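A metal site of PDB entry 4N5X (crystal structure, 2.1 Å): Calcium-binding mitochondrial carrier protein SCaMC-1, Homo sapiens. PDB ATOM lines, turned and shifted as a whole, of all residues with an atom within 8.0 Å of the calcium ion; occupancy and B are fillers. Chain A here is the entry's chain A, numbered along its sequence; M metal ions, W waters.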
ATOM      1  N   PHE A  95       1.498  24.558 -15.840  1.00  0.00           N
ATOM      2  CA  PHE A  95       1.333  23.488 -16.812  1.00  0.00           C
ATOM      3  C   PHE A  95       0.182  23.853 -17.733  1.00  0.00           C
ATOM      4  O   PHE A  95       0.313  23.819 -18.960  1.00  0.00           O
ATOM      5  CB  PHE A  95       1.034  22.169 -16.070  1.00  0.00           C
ATOM      6  CG  PHE A  95       0.923  20.945 -16.958  1.00  0.00           C
ATOM      7  CD1 PHE A  95      -0.260  20.661 -17.623  1.00  0.00           C
ATOM      8  CD2 PHE A  95       1.965  20.030 -17.042  1.00  0.00           C
ATOM      9  CE1 PHE A  95      -0.386  19.504 -18.419  1.00  0.00           C
ATOM     10  CE2 PHE A  95       1.859  18.879 -17.825  1.00  0.00           C
ATOM     11  CZ  PHE A  95       0.685  18.626 -18.518  1.00  0.00           C
ATOM     12  N   LYS A  96      -0.952  24.222 -17.126  1.00  0.00           N
ATOM     13  CA  LYS A  96      -2.163  24.525 -17.876  1.00  0.00           C
ATOM     14  C   LYS A  96      -1.964  25.651 -18.866  1.00  0.00           C
ATOM     15  O   LYS A  96      -2.478  25.612 -19.984  1.00  0.00           O
ATOM     16  CB  LYS A  96      -3.318  24.865 -16.928  1.00  0.00           C
ATOM     17  CG  LYS A  96      -4.177  23.668 -16.524  1.00  0.00           C
ATOM     18  CD  LYS A  96      -5.303  24.117 -15.587  1.00  0.00           C
ATOM     19  CE  LYS A  96      -6.383  23.037 -15.410  1.00  0.00           C
ATOM     20  NZ  LYS A  96      -5.881  21.836 -14.686  1.00  0.00           N
ATOM     21  N   LEU A  98       0.531  26.307 -20.568  1.00  0.00           N
ATOM     22  CA  LEU A  98       1.365  25.883 -21.697  1.00  0.00           C
ATOM     23  C   LEU A  98       0.595  24.905 -22.589  1.00  0.00           C
ATOM     24  O   LEU A  98       0.881  24.777 -23.783  1.00  0.00           O
ATOM     25  CB  LEU A  98       2.654  25.239 -21.179  1.00  0.00           C
ATOM     26  CG  LEU A  98       3.994  25.906 -21.509  1.00  0.00           C
ATOM     27  CD1 LEU A  98       3.951  27.420 -21.328  1.00  0.00           C
ATOM     28  CD2 LEU A  98       5.142  25.284 -20.680  1.00  0.00           C
ATOM     29  N   ASP A  99      -0.380  24.230 -21.993  1.00  0.00           N
ATOM     30  CA  ASP A  99      -1.196  23.237 -22.691  1.00  0.00           C
ATOM     31  C   ASP A  99      -2.281  23.902 -23.548  1.00  0.00           C
ATOM     32  O   ASP A  99      -3.472  23.871 -23.209  1.00  0.00           O
ATOM     33  CB  ASP A  99      -1.824  22.302 -21.657  1.00  0.00           C
ATOM     34  CG  ASP A  99      -2.641  21.183 -22.279  1.00  0.00           C
ATOM     35  OD1 ASP A  99      -2.512  20.946 -23.494  1.00  0.00           O
ATOM     36  OD2 ASP A  99      -3.391  20.536 -21.530  1.00  0.00           O
ATOM     37  N   LYS A 100      -1.868  24.470 -24.674  1.00  0.00           N
ATOM     38  CA  LYS A 100      -2.787  25.232 -25.518  1.00  0.00           C
ATOM     39  C   LYS A 100      -3.979  24.435 -26.051  1.00  0.00           C
ATOM     40  O   LYS A 100      -5.077  24.975 -26.163  1.00  0.00           O
ATOM     41  CB  LYS A 100      -2.035  25.903 -26.672  1.00  0.00           C
ATOM     42  CG  LYS A 100      -1.154  27.054 -26.221  1.00  0.00           C
ATOM     43  CD  LYS A 100      -1.124  28.157 -27.262  1.00  0.00           C
ATOM     44  CE  LYS A 100      -0.993  27.598 -28.662  1.00  0.00           C
ATOM     45  NZ  LYS A 100      -1.158  28.648 -29.698  1.00  0.00           N
ATOM     46  N   ASN A 101      -3.787  23.160 -26.349  1.00  0.00           N
ATOM     47  CA  ASN A 101      -4.895  22.362 -26.898  1.00  0.00           C
ATOM     48  C   ASN A 101      -5.704  21.613 -25.838  1.00  0.00           C
ATOM     49  O   ASN A 101      -6.571  20.818 -26.172  1.00  0.00           O
ATOM     50  CB  ASN A 101      -4.441  21.425 -28.011  1.00  0.00           C
ATOM     51  CG  ASN A 101      -3.575  20.286 -27.505  1.00  0.00           C
ATOM     52  OD1 ASN A 101      -3.377  20.102 -26.298  1.00  0.00           O
ATOM     53  ND2 ASN A 101      -3.056  19.500 -28.438  1.00  0.00           N
ATOM     54  N   ASN A 102      -5.398  21.875 -24.566  1.00  0.00           N
ATOM     55  CA  ASN A 102      -6.174  21.340 -23.442  1.00  0.00           C
ATOM     56  C   ASN A 102      -6.261  19.809 -23.361  1.00  0.00           C
ATOM     57  O   ASN A 102      -7.301  19.267 -22.985  1.00  0.00           O
ATOM     58  CB  ASN A 102      -7.577  21.957 -23.442  1.00  0.00           C
ATOM     59  CG  ASN A 102      -8.262  21.861 -22.093  1.00  0.00           C
ATOM     60  OD1 ASN A 102      -7.609  21.783 -21.056  1.00  0.00           O
ATOM     61  ND2 ASN A 102      -9.587  21.840 -22.103  1.00  0.00           N
ATOM     62  N   ASP A 103      -5.184  19.107 -23.696  1.00  0.00           N
ATOM     63  CA  ASP A 103      -5.234  17.644 -23.647  1.00  0.00           C
ATOM     64  C   ASP A 103      -4.501  17.078 -22.442  1.00  0.00           C
ATOM     65  O   ASP A 103      -4.329  15.862 -22.324  1.00  0.00           O
ATOM     66  CB  ASP A 103      -4.682  17.007 -24.945  1.00  0.00           C
ATOM     67  CG  ASP A 103      -3.193  17.292 -25.171  1.00  0.00           C
ATOM     68  OD1 ASP A 103      -2.523  17.879 -24.290  1.00  0.00           O
ATOM     69  OD2 ASP A 103      -2.693  16.892 -26.246  1.00  0.00           O
ATOM     70  N   GLY A 104      -4.054  17.960 -21.548  1.00  0.00           N
ATOM     71  CA  GLY A 104      -3.316  17.518 -20.378  1.00  0.00           C
ATOM     72  C   GLY A 104      -1.889  17.076 -20.662  1.00  0.00           C
ATOM     73  O   GLY A 104      -1.268  16.439 -19.825  1.00  0.00           O
ATOM     74  N   LYS A 105      -1.370  17.419 -21.839  1.00  0.00           N
ATOM     75  CA  LYS A 105       0.023  17.168 -22.172  1.00  0.00           C
ATOM     76  C   LYS A 105       0.690  18.421 -22.720  1.00  0.00           C
ATOM     77  O   LYS A 105       0.052  19.241 -23.351  1.00  0.00           O
ATOM     78  CB  LYS A 105       0.148  16.040 -23.208  1.00  0.00           C
ATOM     79  CG  LYS A 105      -0.495  14.711 -22.811  1.00  0.00           C
ATOM     80  CD  LYS A 105       0.333  13.989 -21.758  1.00  0.00           C
ATOM     81  CE  LYS A 105      -0.531  13.021 -20.939  1.00  0.00           C
ATOM     82  NZ  LYS A 105      -1.239  12.022 -21.791  1.00  0.00           N
ATOM     83  N   ILE A 106       1.998  18.563 -22.496  1.00  0.00           N
ATOM     84  CA  ILE A 106       2.747  19.629 -23.158  1.00  0.00           C
ATOM     85  C   ILE A 106       3.664  19.068 -24.236  1.00  0.00           C
ATOM     86  O   ILE A 106       4.456  18.159 -23.989  1.00  0.00           O
ATOM     87  CB  ILE A 106       3.547  20.483 -22.132  1.00  0.00           C
ATOM     88  CG1 ILE A 106       2.604  21.175 -21.145  1.00  0.00           C
ATOM     89  CG2 ILE A 106       4.414  21.526 -22.846  1.00  0.00           C
ATOM     90  CD1 ILE A 106       3.319  21.746 -19.942  1.00  0.00           C
ATOM     91  N   GLU A 107       3.530  19.588 -25.450  1.00  0.00           N
ATOM     92  CA  GLU A 107       4.423  19.202 -26.526  1.00  0.00           C
ATOM     93  C   GLU A 107       5.287  20.381 -26.971  1.00  0.00           C
ATOM     94  O   GLU A 107       5.059  21.510 -26.533  1.00  0.00           O
ATOM     95  CB  GLU A 107       3.653  18.586 -27.690  1.00  0.00           C
ATOM     96  CG  GLU A 107       2.547  19.458 -28.238  1.00  0.00           C
ATOM     97  CD  GLU A 107       1.752  18.760 -29.328  1.00  0.00           C
ATOM     98  OE1 GLU A 107       2.334  18.438 -30.386  1.00  0.00           O
ATOM     99  OE2 GLU A 107       0.547  18.505 -29.112  1.00  0.00           O
ATOM    100  N   SER A 109       5.661  22.116 -29.707  1.00  0.00           N
ATOM    101  CA  SER A 109       4.985  23.181 -30.436  1.00  0.00           C
ATOM    102  C   SER A 109       4.199  24.106 -29.494  1.00  0.00           C
ATOM    103  O   SER A 109       4.069  25.295 -29.757  1.00  0.00           O
ATOM    104  CB  SER A 109       4.030  22.573 -31.470  1.00  0.00           C
ATOM    105  OG  SER A 109       2.957  21.918 -30.819  1.00  0.00           O
ATOM    106  N   GLU A 110       3.702  23.563 -28.392  1.00  0.00           N
ATOM    107  CA  GLU A 110       2.960  24.380 -27.446  1.00  0.00           C
ATOM    108  C   GLU A 110       3.878  25.281 -26.652  1.00  0.00           C
ATOM    109  O   GLU A 110       3.505  26.409 -26.331  1.00  0.00           O
ATOM    110  CB  GLU A 110       2.103  23.515 -26.511  1.00  0.00           C
ATOM    111  CG  GLU A 110       1.030  22.753 -27.235  1.00  0.00           C
ATOM    112  CD  GLU A 110       0.206  21.874 -26.325  1.00  0.00           C
ATOM    113  OE1 GLU A 110       0.796  21.169 -25.486  1.00  0.00           O
ATOM    114  OE2 GLU A 110      -1.038  21.910 -26.461  1.00  0.00           O
ATOM    115  N   THR A 141       6.239  14.092 -24.903  1.00  0.00           N
ATOM    116  CA  THR A 141       5.132  14.844 -24.348  1.00  0.00           C
ATOM    117  C   THR A 141       5.383  14.857 -22.850  1.00  0.00           C
ATOM    118  O   THR A 141       5.847  13.875 -22.307  1.00  0.00           O
ATOM    119  CB  THR A 141       3.781  14.166 -24.620  1.00  0.00           C
ATOM    120  OG1 THR A 141       3.753  12.876 -24.002  1.00  0.00           O
ATOM    121  CG2 THR A 141       3.558  13.988 -26.129  1.00  0.00           C
ATOM    122  N   VAL A 142       5.094  15.971 -22.190  1.00  0.00           N
ATOM    123  CA  VAL A 142       5.268  16.028 -20.745  1.00  0.00           C
ATOM    124  C   VAL A 142       3.915  15.899 -20.083  1.00  0.00           C
ATOM    125  O   VAL A 142       3.019  16.684 -20.374  1.00  0.00           O
ATOM    126  CB  VAL A 142       5.919  17.353 -20.287  1.00  0.00           C
ATOM    127  CG1 VAL A 142       5.801  17.529 -18.767  1.00  0.00           C
ATOM    128  CG2 VAL A 142       7.367  17.437 -20.761  1.00  0.00           C
HETATM  129 CA    CA M   1      -1.273  19.915 -25.082  1.00  0.00          CA
HETATM  130  O   HOH W   1      -0.529  18.331 -26.737  1.00  0.00           O
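The calcium ion is bound by OD1 of Asp 99, O of Lys 105, water W1, OE2 of Glu 110, OD1 of Asn 101, OE1 of Glu 110 and OD1 of Asp 103.
Water W1 lies within hydrogen-bond range of OE2 of Glu 107, OD2 of Asp 103 and ND2 of Asn 101.
The side-chain carboxylate of Asp 99 sits close to the backbone NH of Asn 102.
OD2 of Asp 99 is in hydrogen-bond range of N of Gly 104 (2.7 Å).
OE2 of Glu 110 lies close to N of Lys 100 (3.2 Å).
OE1 of Glu 110 sits close to N of Glu 107 (3.2 Å).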
